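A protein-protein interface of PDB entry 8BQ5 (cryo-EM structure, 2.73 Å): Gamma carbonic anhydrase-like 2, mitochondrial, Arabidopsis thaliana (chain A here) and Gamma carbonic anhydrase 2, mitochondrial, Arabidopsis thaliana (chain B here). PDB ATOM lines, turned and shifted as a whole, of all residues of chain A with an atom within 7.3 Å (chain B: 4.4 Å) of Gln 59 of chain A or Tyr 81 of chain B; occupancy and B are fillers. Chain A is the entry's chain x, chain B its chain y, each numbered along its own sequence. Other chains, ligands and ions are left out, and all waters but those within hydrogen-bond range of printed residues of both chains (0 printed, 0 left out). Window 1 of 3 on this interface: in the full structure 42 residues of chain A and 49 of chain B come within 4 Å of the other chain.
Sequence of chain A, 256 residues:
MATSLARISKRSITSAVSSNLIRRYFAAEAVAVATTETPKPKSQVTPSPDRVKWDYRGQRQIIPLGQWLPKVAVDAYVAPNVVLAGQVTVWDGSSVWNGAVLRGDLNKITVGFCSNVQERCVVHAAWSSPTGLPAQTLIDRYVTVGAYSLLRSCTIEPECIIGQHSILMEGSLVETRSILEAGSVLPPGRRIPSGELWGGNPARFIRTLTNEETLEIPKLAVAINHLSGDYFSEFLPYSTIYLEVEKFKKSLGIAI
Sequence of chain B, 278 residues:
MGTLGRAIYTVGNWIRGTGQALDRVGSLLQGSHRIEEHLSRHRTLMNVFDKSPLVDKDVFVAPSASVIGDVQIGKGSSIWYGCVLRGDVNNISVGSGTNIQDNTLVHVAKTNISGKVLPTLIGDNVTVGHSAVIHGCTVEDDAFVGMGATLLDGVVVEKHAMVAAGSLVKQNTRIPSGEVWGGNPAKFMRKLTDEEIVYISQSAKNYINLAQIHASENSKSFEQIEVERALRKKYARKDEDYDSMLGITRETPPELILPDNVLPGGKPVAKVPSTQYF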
ATOM      1  N   ASP A  55      28.288   4.416 -18.724  1.00  0.00           N
ATOM      2  CA  ASP A  55      29.555   4.190 -19.408  1.00  0.00           C
ATOM      3  C   ASP A  55      29.348   4.502 -20.886  1.00  0.00           C
ATOM      4  O   ASP A  55      28.587   3.811 -21.570  1.00  0.00           O
ATOM      5  CB  ASP A  55      30.026   2.753 -19.197  1.00  0.00           C
ATOM      6  CG  ASP A  55      31.489   2.560 -19.534  1.00  0.00           C
ATOM      7  OD1 ASP A  55      31.897   2.912 -20.660  1.00  0.00           O
ATOM      8  OD2 ASP A  55      32.231   2.051 -18.668  1.00  0.00           O
ATOM      9  N   TYR A  56      30.028   5.542 -21.375  1.00  0.00           N
ATOM     10  CA  TYR A  56      29.838   5.985 -22.753  1.00  0.00           C
ATOM     11  C   TYR A  56      30.283   4.942 -23.768  1.00  0.00           C
ATOM     12  O   TYR A  56      29.860   5.002 -24.926  1.00  0.00           O
ATOM     13  CB  TYR A  56      30.591   7.298 -22.989  1.00  0.00           C
ATOM     14  CG  TYR A  56      32.084   7.124 -23.143  1.00  0.00           C
ATOM     15  CD1 TYR A  56      32.916   7.128 -22.036  1.00  0.00           C
ATOM     16  CD2 TYR A  56      32.663   6.960 -24.395  1.00  0.00           C
ATOM     17  CE1 TYR A  56      34.276   6.967 -22.170  1.00  0.00           C
ATOM     18  CE2 TYR A  56      34.023   6.796 -24.535  1.00  0.00           C
ATOM     19  CZ  TYR A  56      34.825   6.802 -23.417  1.00  0.00           C
ATOM     20  OH  TYR A  56      36.184   6.642 -23.540  1.00  0.00           O
ATOM     21  N   ARG A  57      31.137   4.000 -23.370  1.00  0.00           N
ATOM     22  CA  ARG A  57      31.597   2.969 -24.290  1.00  0.00           C
ATOM     23  C   ARG A  57      30.596   1.835 -24.450  1.00  0.00           C
ATOM     24  O   ARG A  57      30.723   1.047 -25.392  1.00  0.00           O
ATOM     25  CB  ARG A  57      32.936   2.400 -23.824  1.00  0.00           C
ATOM     26  CG  ARG A  57      33.916   3.453 -23.356  1.00  0.00           C
ATOM     27  CD  ARG A  57      35.059   2.849 -22.570  1.00  0.00           C
ATOM     28  NE  ARG A  57      34.676   2.510 -21.206  1.00  0.00           N
ATOM     29  CZ  ARG A  57      35.511   2.022 -20.299  1.00  0.00           C
ATOM     30  NH1 ARG A  57      36.789   1.826 -20.574  1.00  0.00           N
ATOM     31  NH2 ARG A  57      35.053   1.731 -19.085  1.00  0.00           N
ATOM     32  N   GLY A  58      29.611   1.742 -23.567  1.00  0.00           N
ATOM     33  CA  GLY A  58      28.717   0.604 -23.561  1.00  0.00           C
ATOM     34  C   GLY A  58      29.411  -0.629 -23.010  1.00  0.00           C
ATOM     35  O   GLY A  58      30.470  -0.569 -22.393  1.00  0.00           O
ATOM     36  N   GLN A  59      28.785  -1.773 -23.254  1.00  0.00           N
ATOM     37  CA  GLN A  59      29.336  -3.048 -22.816  1.00  0.00           C
ATOM     38  C   GLN A  59      30.346  -3.545 -23.842  1.00  0.00           C
ATOM     39  O   GLN A  59      30.031  -3.646 -25.032  1.00  0.00           O
ATOM     40  CB  GLN A  59      28.213  -4.064 -22.624  1.00  0.00           C
ATOM     41  CG  GLN A  59      28.688  -5.490 -22.453  1.00  0.00           C
ATOM     42  CD  GLN A  59      29.372  -5.713 -21.124  1.00  0.00           C
ATOM     43  OE1 GLN A  59      28.783  -5.491 -20.070  1.00  0.00           O
ATOM     44  NE2 GLN A  59      30.619  -6.164 -21.166  1.00  0.00           N
ATOM     45  N   ARG A  60      31.560  -3.846 -23.385  1.00  0.00           N
ATOM     46  CA  ARG A  60      32.569  -4.418 -24.267  1.00  0.00           C
ATOM     47  C   ARG A  60      32.128  -5.796 -24.738  1.00  0.00           C
ATOM     48  O   ARG A  60      31.653  -6.615 -23.946  1.00  0.00           O
ATOM     49  CB  ARG A  60      33.914  -4.509 -23.548  1.00  0.00           C
ATOM     50  CG  ARG A  60      34.991  -3.623 -24.139  1.00  0.00           C
ATOM     51  CD  ARG A  60      36.370  -4.021 -23.653  1.00  0.00           C
ATOM     52  NE  ARG A  60      36.527  -3.860 -22.214  1.00  0.00           N
ATOM     53  CZ  ARG A  60      37.433  -4.501 -21.490  1.00  0.00           C
ATOM     54  NH1 ARG A  60      38.265  -5.369 -22.039  1.00  0.00           N
ATOM     55  NH2 ARG A  60      37.509  -4.262 -20.185  1.00  0.00           N
ATOM     56  N   GLN A  61      32.283  -6.052 -26.038  1.00  0.00           N
ATOM     57  CA  GLN A  61      31.846  -7.329 -26.591  1.00  0.00           C
ATOM     58  C   GLN A  61      32.780  -8.463 -26.190  1.00  0.00           C
ATOM     59  O   GLN A  61      32.321  -9.548 -25.811  1.00  0.00           O
ATOM     60  CB  GLN A  61      31.743  -7.231 -28.111  1.00  0.00           C
ATOM     61  CG  GLN A  61      31.222  -8.489 -28.776  1.00  0.00           C
ATOM     62  CD  GLN A  61      31.268  -8.409 -30.285  1.00  0.00           C
ATOM     63  OE1 GLN A  61      32.339  -8.297 -30.879  1.00  0.00           O
ATOM     64  NE2 GLN A  61      30.103  -8.456 -30.915  1.00  0.00           N
ATOM     65  N   ILE A  62      34.087  -8.240 -26.270  1.00  0.00           N
ATOM     66  CA  ILE A  62      35.086  -9.258 -25.972  1.00  0.00           C
ATOM     67  C   ILE A  62      35.640  -8.964 -24.587  1.00  0.00           C
ATOM     68  O   ILE A  62      36.248  -7.911 -24.363  1.00  0.00           O
ATOM     69  CB  ILE A  62      36.207  -9.286 -27.020  1.00  0.00           C
ATOM     70  CG1 ILE A  62      35.638  -9.533 -28.420  1.00  0.00           C
ATOM     71  CG2 ILE A  62      37.242 -10.334 -26.659  1.00  0.00           C
ATOM     72  CD1 ILE A  62      34.944 -10.858 -28.574  1.00  0.00           C
ATOM     73  N   ILE A  63      35.441  -9.892 -23.659  1.00  0.00           N
ATOM     74  CA  ILE A  63      35.917  -9.717 -22.291  1.00  0.00           C
ATOM     75  C   ILE A  63      37.031 -10.725 -22.031  1.00  0.00           C
ATOM     76  O   ILE A  63      36.753 -11.910 -21.803  1.00  0.00           O
ATOM     77  CB  ILE A  63      34.773  -9.869 -21.275  1.00  0.00           C
ATOM     78  CG1 ILE A  63      33.729  -8.768 -21.475  1.00  0.00           C
ATOM     79  CG2 ILE A  63      35.309  -9.843 -19.851  1.00  0.00           C
ATOM     80  CD1 ILE A  63      34.186  -7.402 -21.017  1.00  0.00           C
ATOM     81  N   LEU A  65      39.867 -12.595 -19.775  1.00  0.00           N
ATOM     82  CA  LEU A  65      39.962 -12.952 -18.358  1.00  0.00           C
ATOM     83  C   LEU A  65      41.373 -13.499 -18.153  1.00  0.00           C
ATOM     84  O   LEU A  65      41.626 -14.688 -18.363  1.00  0.00           O
ATOM     85  CB  LEU A  65      38.889 -13.957 -17.962  1.00  0.00           C
ATOM     86  CG  LEU A  65      37.444 -13.446 -17.955  1.00  0.00           C
ATOM     87  CD1 LEU A  65      36.482 -14.574 -17.631  1.00  0.00           C
ATOM     88  CD2 LEU A  65      37.275 -12.302 -16.967  1.00  0.00           C
ATOM     89  N   PRO A  80      26.457  -7.171 -32.379  1.00  0.00           N
ATOM     90  CA  PRO A  80      27.174  -6.150 -31.593  1.00  0.00           C
ATOM     91  C   PRO A  80      26.965  -6.245 -30.089  1.00  0.00           C
ATOM     92  O   PRO A  80      27.910  -6.000 -29.330  1.00  0.00           O
ATOM     93  CB  PRO A  80      26.622  -4.835 -32.159  1.00  0.00           C
ATOM     94  CG  PRO A  80      26.185  -5.175 -33.536  1.00  0.00           C
ATOM     95  CD  PRO A  80      25.653  -6.572 -33.459  1.00  0.00           C
ATOM     96  N   ASN A  81      25.768  -6.597 -29.625  1.00  0.00           N
ATOM     97  CA  ASN A  81      25.483  -6.598 -28.196  1.00  0.00           C
ATOM     98  C   ASN A  81      25.735  -7.951 -27.536  1.00  0.00           C
ATOM     99  O   ASN A  81      25.381  -8.132 -26.367  1.00  0.00           O
ATOM    100  CB  ASN A  81      24.046  -6.131 -27.940  1.00  0.00           C
ATOM    101  CG  ASN A  81      23.007  -7.114 -28.431  1.00  0.00           C
ATOM    102  OD1 ASN A  81      23.278  -7.951 -29.290  1.00  0.00           O
ATOM    103  ND2 ASN A  81      21.800  -7.007 -27.893  1.00  0.00           N
ATOM    104  N   VAL A  82      26.339  -8.896 -28.256  1.00  0.00           N
ATOM    105  CA  VAL A  82      26.745 -10.164 -27.665  1.00  0.00           C
ATOM    106  C   VAL A  82      27.919  -9.939 -26.718  1.00  0.00           C
ATOM    107  O   VAL A  82      28.762  -9.061 -26.934  1.00  0.00           O
ATOM    108  CB  VAL A  82      27.109 -11.166 -28.777  1.00  0.00           C
ATOM    109  CG1 VAL A  82      27.792 -12.401 -28.213  1.00  0.00           C
ATOM    110  CG2 VAL A  82      25.876 -11.555 -29.563  1.00  0.00           C
ATOM    111  N   VAL A  83      27.974 -10.730 -25.650  1.00  0.00           N
ATOM    112  CA  VAL A  83      29.122 -10.759 -24.753  1.00  0.00           C
ATOM    113  C   VAL A  83      29.790 -12.122 -24.881  1.00  0.00           C
ATOM    114  O   VAL A  83      29.136 -13.160 -24.723  1.00  0.00           O
ATOM    115  CB  VAL A  83      28.722 -10.477 -23.297  1.00  0.00           C
ATOM    116  CG1 VAL A  83      29.916 -10.668 -22.377  1.00  0.00           C
ATOM    117  CG2 VAL A  83      28.167  -9.072 -23.163  1.00  0.00           C
ATOM    118  N   LEU A  84      31.084 -12.117 -25.192  1.00  0.00           N
ATOM    119  CA  LEU A  84      31.935 -13.297 -25.110  1.00  0.00           C
ATOM    120  C   LEU A  84      32.985 -13.034 -24.041  1.00  0.00           C
ATOM    121  O   LEU A  84      33.697 -12.027 -24.105  1.00  0.00           O
ATOM    122  CB  LEU A  84      32.611 -13.605 -26.448  1.00  0.00           C
ATOM    123  CG  LEU A  84      31.807 -13.616 -27.747  1.00  0.00           C
ATOM    124  CD1 LEU A  84      32.751 -13.822 -28.913  1.00  0.00           C
ATOM    125  CD2 LEU A  84      30.735 -14.691 -27.739  1.00  0.00           C
ATOM    126  N   ALA A  85      33.083 -13.928 -23.063  1.00  0.00           N
ATOM    127  CA  ALA A  85      34.030 -13.766 -21.969  1.00  0.00           C
ATOM    128  C   ALA A  85      34.811 -15.055 -21.768  1.00  0.00           C
ATOM    129  O   ALA A  85      34.222 -16.139 -21.711  1.00  0.00           O
ATOM    130  CB  ALA A  85      33.314 -13.368 -20.675  1.00  0.00           C
ATOM    131  N   GLY A  99      21.846 -10.462 -28.105  1.00  0.00           N
ATOM    132  CA  GLY A  99      21.534 -10.734 -26.722  1.00  0.00           C
ATOM    133  C   GLY A  99      22.116 -12.011 -26.167  1.00  0.00           C
ATOM    134  O   GLY A  99      21.892 -12.312 -24.988  1.00  0.00           O
ATOM    135  N   ALA A 100      22.853 -12.772 -26.969  1.00  0.00           N
ATOM    136  CA  ALA A 100      23.455 -14.005 -26.495  1.00  0.00           C
ATOM    137  C   ALA A 100      24.662 -13.711 -25.615  1.00  0.00           C
ATOM    138  O   ALA A 100      25.387 -12.734 -25.819  1.00  0.00           O
ATOM    139  CB  ALA A 100      23.863 -14.892 -27.671  1.00  0.00           C
ATOM    140  N   VAL A 101      24.867 -14.569 -24.620  1.00  0.00           N
ATOM    141  CA  VAL A 101      25.952 -14.434 -23.656  1.00  0.00           C
ATOM    142  C   VAL A 101      26.708 -15.753 -23.617  1.00  0.00           C
ATOM    143  O   VAL A 101      26.119 -16.800 -23.326  1.00  0.00           O
ATOM    144  CB  VAL A 101      25.433 -14.064 -22.255  1.00  0.00           C
ATOM    145  CG1 VAL A 101      26.580 -13.986 -21.258  1.00  0.00           C
ATOM    146  CG2 VAL A 101      24.668 -12.752 -22.299  1.00  0.00           C
ATOM    147  N   LEU A 102      28.005 -15.708 -23.912  1.00  0.00           N
ATOM    148  CA  LEU A 102      28.865 -16.887 -23.897  1.00  0.00           C
ATOM    149  C   LEU A 102      29.979 -16.638 -22.892  1.00  0.00           C
ATOM    150  O   LEU A 102      30.938 -15.917 -23.187  1.00  0.00           O
ATOM    151  CB  LEU A 102      29.427 -17.182 -25.286  1.00  0.00           C
ATOM    152  CG  LEU A 102      28.508 -17.879 -26.298  1.00  0.00           C
ATOM    153  CD1 LEU A 102      27.409 -16.959 -26.792  1.00  0.00           C
ATOM    154  CD2 LEU A 102      29.318 -18.396 -27.466  1.00  0.00           C
ATOM    155  N   ARG A 103      29.807 -17.241 -21.717  1.00  0.00           N
ATOM    156  CA  ARG A 103      30.742 -16.973 -20.602  1.00  0.00           C
ATOM    157  C   ARG A 103      31.611 -18.201 -20.330  1.00  0.00           C
ATOM    158  O   ARG A 103      31.133 -19.139 -19.686  1.00  0.00           O
ATOM    159  CB  ARG A 103      29.928 -16.515 -19.388  1.00  0.00           C
ATOM    160  CG  ARG A 103      30.773 -16.042 -18.218  1.00  0.00           C
ATOM    161  CD  ARG A 103      30.081 -15.010 -17.349  1.00  0.00           C
ATOM    162  NE  ARG A 103      28.787 -15.428 -16.838  1.00  0.00           N
ATOM    163  CZ  ARG A 103      28.589 -16.060 -15.687  1.00  0.00           C
ATOM    164  NH1 ARG A 103      29.611 -16.365 -14.908  1.00  0.00           N
ATOM    165  NH2 ARG A 103      27.363 -16.384 -15.320  1.00  0.00           N
ATOM    166  N   ASP A 105      34.272 -18.750 -18.257  1.00  0.00           N
ATOM    167  CA  ASP A 105      35.162 -18.477 -17.135  1.00  0.00           C
ATOM    168  C   ASP A 105      35.440 -19.697 -16.269  1.00  0.00           C
ATOM    169  O   ASP A 105      36.413 -19.685 -15.509  1.00  0.00           O
ATOM    170  CB  ASP A 105      34.604 -17.350 -16.254  1.00  0.00           C
ATOM    171  CG  ASP A 105      33.114 -17.465 -16.025  1.00  0.00           C
ATOM    172  OD1 ASP A 105      32.544 -18.543 -16.290  1.00  0.00           O
ATOM    173  OD2 ASP A 105      32.514 -16.474 -15.561  1.00  0.00           O
ATOM    174  N   ARG A 120      19.439 -14.301 -27.579  1.00  0.00           N
ATOM    175  CA  ARG A 120      19.238 -14.366 -26.131  1.00  0.00           C
ATOM    176  C   ARG A 120      19.511 -15.748 -25.551  1.00  0.00           C
ATOM    177  O   ARG A 120      18.993 -16.092 -24.486  1.00  0.00           O
ATOM    178  CB  ARG A 120      17.833 -13.888 -25.749  1.00  0.00           C
ATOM    179  CG  ARG A 120      17.577 -12.451 -26.182  1.00  0.00           C
ATOM    180  CD  ARG A 120      16.623 -11.699 -25.269  1.00  0.00           C
ATOM    181  NE  ARG A 120      16.949 -11.838 -23.855  1.00  0.00           N
ATOM    182  CZ  ARG A 120      17.682 -10.976 -23.165  1.00  0.00           C
ATOM    183  NH1 ARG A 120      18.238  -9.923 -23.740  1.00  0.00           N
ATOM    184  NH2 ARG A 120      17.866 -11.179 -21.864  1.00  0.00           N
ATOM    185  N   VAL A 122      21.962 -18.264 -23.545  1.00  0.00           N
ATOM    186  CA  VAL A 122      23.035 -18.191 -22.564  1.00  0.00           C
ATOM    187  C   VAL A 122      23.786 -19.509 -22.616  1.00  0.00           C
ATOM    188  O   VAL A 122      23.193 -20.577 -22.428  1.00  0.00           O
ATOM    189  CB  VAL A 122      22.516 -17.906 -21.147  1.00  0.00           C
ATOM    190  CG1 VAL A 122      23.679 -17.808 -20.178  1.00  0.00           C
ATOM    191  CG2 VAL A 122      21.708 -16.624 -21.130  1.00  0.00           C
ATOM    192  N   PHE B  60      29.505  -6.372  -8.168  1.00  0.00           N
ATOM    193  CA  PHE B  60      29.721  -6.388  -9.606  1.00  0.00           C
ATOM    194  C   PHE B  60      28.393  -6.163 -10.310  1.00  0.00           C
ATOM    195  O   PHE B  60      27.488  -6.998 -10.228  1.00  0.00           O
ATOM    196  CB  PHE B  60      30.341  -7.702 -10.070  1.00  0.00           C
ATOM    197  CG  PHE B  60      30.393  -7.840 -11.565  1.00  0.00           C
ATOM    198  CD1 PHE B  60      30.905  -6.819 -12.350  1.00  0.00           C
ATOM    199  CD2 PHE B  60      29.903  -8.971 -12.188  1.00  0.00           C
ATOM    200  CE1 PHE B  60      30.946  -6.937 -13.724  1.00  0.00           C
ATOM    201  CE2 PHE B  60      29.941  -9.091 -13.565  1.00  0.00           C
ATOM    202  CZ  PHE B  60      30.464  -8.073 -14.331  1.00  0.00           C
ATOM    203  N   ALA B  62      27.367  -5.698 -14.129  1.00  0.00           N
ATOM    204  CA  ALA B  62      27.825  -5.689 -15.506  1.00  0.00           C
ATOM    205  C   ALA B  62      27.373  -4.396 -16.176  1.00  0.00           C
ATOM    206  O   ALA B  62      26.281  -3.897 -15.885  1.00  0.00           O
ATOM    207  CB  ALA B  62      27.279  -6.898 -16.266  1.00  0.00           C
ATOM    208  N   PRO B  63      28.198  -3.807 -17.040  1.00  0.00           N
ATOM    209  CA  PRO B  63      27.760  -2.594 -17.747  1.00  0.00           C
ATOM    210  C   PRO B  63      26.490  -2.796 -18.555  1.00  0.00           C
ATOM    211  O   PRO B  63      25.701  -1.854 -18.689  1.00  0.00           O
ATOM    212  CB  PRO B  63      28.960  -2.260 -18.641  1.00  0.00           C
ATOM    213  CG  PRO B  63      30.126  -2.870 -17.939  1.00  0.00           C
ATOM    214  CD  PRO B  63      29.614  -4.121 -17.296  1.00  0.00           C
ATOM    215  N   SER B  64      26.260  -3.996 -19.087  1.00  0.00           N
ATOM    216  CA  SER B  64      25.063  -4.262 -19.874  1.00  0.00           C
ATOM    217  C   SER B  64      23.826  -4.504 -19.020  1.00  0.00           C
ATOM    218  O   SER B  64      22.721  -4.570 -19.570  1.00  0.00           O
ATOM    219  CB  SER B  64      25.284  -5.467 -20.789  1.00  0.00           C
ATOM    220  OG  SER B  64      25.925  -6.522 -20.100  1.00  0.00           O
ATOM    221  N   TRP B  80      24.820  -9.881 -13.342  1.00  0.00           N
ATOM    222  CA  TRP B  80      25.566 -10.282 -14.559  1.00  0.00           C
ATOM    223  C   TRP B  80      25.080  -9.640 -15.855  1.00  0.00           C
ATOM    224  O   TRP B  80      24.246  -8.735 -15.803  1.00  0.00           O
ATOM    225  CB  TRP B  80      25.631 -11.813 -14.609  1.00  0.00           C
ATOM    226  CG  TRP B  80      26.488 -12.319 -13.493  1.00  0.00           C
ATOM    227  CD1 TRP B  80      26.112 -12.561 -12.204  1.00  0.00           C
ATOM    228  CD2 TRP B  80      27.904 -12.551 -13.548  1.00  0.00           C
ATOM    229  NE1 TRP B  80      27.190 -12.966 -11.465  1.00  0.00           N
ATOM    230  CE2 TRP B  80      28.303 -12.966 -12.261  1.00  0.00           C
ATOM    231  CE3 TRP B  80      28.862 -12.472 -14.563  1.00  0.00           C
ATOM    232  CZ2 TRP B  80      29.623 -13.300 -11.965  1.00  0.00           C
ATOM    233  CZ3 TRP B  80      30.164 -12.802 -14.267  1.00  0.00           C
ATOM    234  CH2 TRP B  80      30.536 -13.211 -12.987  1.00  0.00           C
ATOM    235  N   TYR B  81      25.598 -10.122 -16.976  1.00  0.00           N
ATOM    236  CA  TYR B  81      25.367  -9.480 -18.265  1.00  0.00           C
ATOM    237  C   TYR B  81      23.915  -9.621 -18.703  1.00  0.00           C
ATOM    238  O   TYR B  81      23.344 -10.713 -18.667  1.00  0.00           O
ATOM    239  CB  TYR B  81      26.302 -10.080 -19.314  1.00  0.00           C
ATOM    240  CG  TYR B  81      27.755 -10.004 -18.923  1.00  0.00           C
ATOM    241  CD1 TYR B  81      28.460  -8.815 -19.039  1.00  0.00           C
ATOM    242  CD2 TYR B  81      28.418 -11.112 -18.414  1.00  0.00           C
ATOM    243  CE1 TYR B  81      29.784  -8.733 -18.674  1.00  0.00           C
ATOM    244  CE2 TYR B  81      29.745 -11.040 -18.045  1.00  0.00           C
ATOM    245  CZ  TYR B  81      30.423  -9.847 -18.178  1.00  0.00           C
ATOM    246  OH  TYR B  81      31.744  -9.763 -17.816  1.00  0.00           O
ATOM    247  N   GLY B  82      23.321  -8.506 -19.122  1.00  0.00           N
ATOM    248  CA  GLY B  82      21.966  -8.505 -19.626  1.00  0.00           C
ATOM    249  C   GLY B  82      20.880  -8.585 -18.576  1.00  0.00           C
ATOM    250  O   GLY B  82      19.705  -8.715 -18.938  1.00  0.00           O
ATOM    251  N   CYS B  83      21.227  -8.512 -17.296  1.00  0.00           N
ATOM    252  CA  CYS B  83      20.223  -8.577 -16.246  1.00  0.00           C
ATOM    253  C   CYS B  83      19.445  -7.272 -16.158  1.00  0.00           C
ATOM    254  O   CYS B  83      20.001  -6.178 -16.287  1.00  0.00           O
ATOM    255  CB  CYS B  83      20.873  -8.875 -14.900  1.00  0.00           C
ATOM    256  SG  CYS B  83      21.444 -10.560 -14.726  1.00  0.00           S
ATOM    257  N   ASP B 102      23.272 -14.228 -15.815  1.00  0.00           N
ATOM    258  CA  ASP B 102      23.006 -13.613 -17.140  1.00  0.00           C
ATOM    259  C   ASP B 102      21.573 -13.619 -17.650  1.00  0.00           C
ATOM    260  O   ASP B 102      20.901 -14.662 -17.535  1.00  0.00           O
ATOM    261  CB  ASP B 102      23.863 -14.300 -18.210  1.00  0.00           C
ATOM    262  CG  ASP B 102      25.339 -14.364 -17.861  1.00  0.00           C
ATOM    263  OD1 ASP B 102      25.897 -13.318 -17.477  1.00  0.00           O
ATOM    264  OD2 ASP B 102      25.918 -15.462 -17.972  1.00  0.00           O
ATOM    265  N   ASN B 103      21.150 -12.478 -18.193  1.00  0.00           N
ATOM    266  CA  ASN B 103      19.873 -12.375 -18.902  1.00  0.00           C
ATOM    267  C   ASN B 103      18.668 -12.618 -17.998  1.00  0.00           C
ATOM    268  O   ASN B 103      17.607 -13.029 -18.478  1.00  0.00           O
ATOM    269  CB  ASN B 103      19.822 -13.328 -20.102  1.00  0.00           C
ATOM    270  CG  ASN B 103      20.562 -12.790 -21.314  1.00  0.00           C
ATOM    271  OD1 ASN B 103      21.070 -11.671 -21.302  1.00  0.00           O
ATOM    272  ND2 ASN B 103      20.613 -13.587 -22.374  1.00  0.00           N
ATOM    273  N   HIS B 214      35.453 -10.484 -13.059  1.00  0.00           N
ATOM    274  CA  HIS B 214      34.655  -9.794 -14.070  1.00  0.00           C
ATOM    275  C   HIS B 214      34.561  -8.295 -13.787  1.00  0.00           C
ATOM    276  O   HIS B 214      34.635  -7.476 -14.713  1.00  0.00           O
ATOM    277  CB  HIS B 214      33.274 -10.431 -14.176  1.00  0.00           C
ATOM    278  CG  HIS B 214      33.262 -11.683 -14.993  1.00  0.00           C
ATOM    279  ND1 HIS B 214      32.990 -11.688 -16.344  1.00  0.00           N
ATOM    280  CD2 HIS B 214      33.513 -12.969 -14.656  1.00  0.00           C
ATOM    281  CE1 HIS B 214      33.060 -12.925 -16.800  1.00  0.00           C
ATOM    282  NE2 HIS B 214      33.374 -13.722 -15.795  1.00  0.00           N
ATOM    283  N   ASN B 218      35.877  -5.351 -16.361  1.00  0.00           N
ATOM    284  CA  ASN B 218      34.925  -4.431 -16.977  1.00  0.00           C
ATOM    285  C   ASN B 218      35.180  -2.970 -16.622  1.00  0.00           C
ATOM    286  O   ASN B 218      34.638  -2.084 -17.290  1.00  0.00           O
ATOM    287  CB  ASN B 218      33.499  -4.817 -16.590  1.00  0.00           C
ATOM    288  CG  ASN B 218      32.909  -5.846 -17.527  1.00  0.00           C
ATOM    289  OD1 ASN B 218      32.362  -5.505 -18.573  1.00  0.00           O
ATOM    290  ND2 ASN B 218      33.027  -7.115 -17.162  1.00  0.00           N
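The side-chain amide oxygen of Gln 59 of chain A lies within hydrogen-bond range of the side-chain hydroxyl of Ser 64 of chain B (3.0 Å).
The side-chain amide nitrogen (NE2) of Gln 59 of chain A sits at hydrogen-bond distance from the side-chain amide oxygen (OD1) of Asn 218 of chain B, at 3.2 Å.
The backbone carbonyl oxygen (O) of Gly 99 of chain A sits at hydrogen-bond distance from the side-chain amide nitrogen (ND2) of Asn 103 of chain B (3.2 Å).
The guanidinium group of Arg 103 of chain A is in salt-bridge range of the side-chain carboxylate of Asp 102 of chain B, at 3.1 Å.
NE2 of His 214 of chain B is in hydrogen-bond range of OD2 of Asp 105 of chain A, at 2.9 Å.
The guanidinium group (NH2) of Arg 120 of chain A sits close to the side-chain amide oxygen (OD1) of Asn 103 of chain B.
The backbone NH of Ile 63 of chain A is in hydrogen-bond range of the backbone carbonyl oxygen of Leu 84 of chain A.
The side-chain amide oxygen (OD1) of Asn 81 of chain A sits at hydrogen-bond distance from the backbone NH (N) of Gly 99 of chain A, at 3.1 Å.
The side-chain carboxylate of Asp 105 of chain A is in salt-bridge range of the guanidinium group of Arg 103 of chain A (3.0 Å).
OG of Ser 64 of chain B sits at hydrogen-bond distance from N of Gly 82 of chain B (3.4 Å).
The side-chain sulfur (SG) of Cys 83 of chain B lies close to the backbone carbonyl oxygen (O) of Trp 80 of chain B, 3.5 Å away.
The side-chain hydroxyl of Tyr 81 of chain B lies within hydrogen-bond range of the side-chain amide nitrogen of Asn 218 of chain B (3.0 Å).
Gln 59 of chain A touches Pro 63 of chain B.
OE1 of Gln 59 of chain A touches CD1 of Tyr 81 of chain B, 3.5 Å away.
Asn 218 of chain B touches Ile 63 of chain A (OD1 to CD1, 3.6 Å).
Leu 65 of chain A touches His 214 of chain B.
His 214 of chain B touches Ala 85 of chain A.
Val 101 of chain A touches Asn 103 of chain B (CG2 to OD1, 3.9 Å).
Arg 103 of chain A touches Trp 80 of chain B.
His 214 of chain B touches Arg 103 of chain A.
Val 122 of chain A touches Asp 102 of chain B (CG1 to OD2, 3.9 Å).
CG2 of Val 122 of chain A touches ND2 of Asn 103 of chain B, at 3.5 Å.
Gln 59 of chain A touches four residues of chain B.
Val 82 of chain A touches none of the printed residues of chain B.
Of the printed residues of chain B, Gly 99 of chain A touches Asn 103.
Tyr 81 of chain B touches just one residue of chain A: Gln 59 (3.5 Å).
Cys 83 of chain B touches none of the printed residues of chain A.
Printed residues of chain A within 4 Å of Asp 102 of chain B: Val 101 (3.6 Å), Arg 103 (3.1 Å) and Val 122 (3.9 Å).
Printed residues of chain A within 4 Å of Asn 218 of chain B: Gln 59 (3.2 Å) and Ile 63 (3.6 Å).
Along chain A the printed residues that touch a printed residue of chain B span positions 59 to 122.
Of the 12 printed residues of chain B, 8 touch a printed residue of chain A.
Hydrophobic or aromatic side chains of chain B within 4 Å of the printed part of chain A: Pro 63, Trp 80, Tyr 81 and His 214.
Along chain B the printed residues that touch a printed residue of chain A span positions 63 to 218.
Among the printed residues, 17 pairs touch across the chains.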
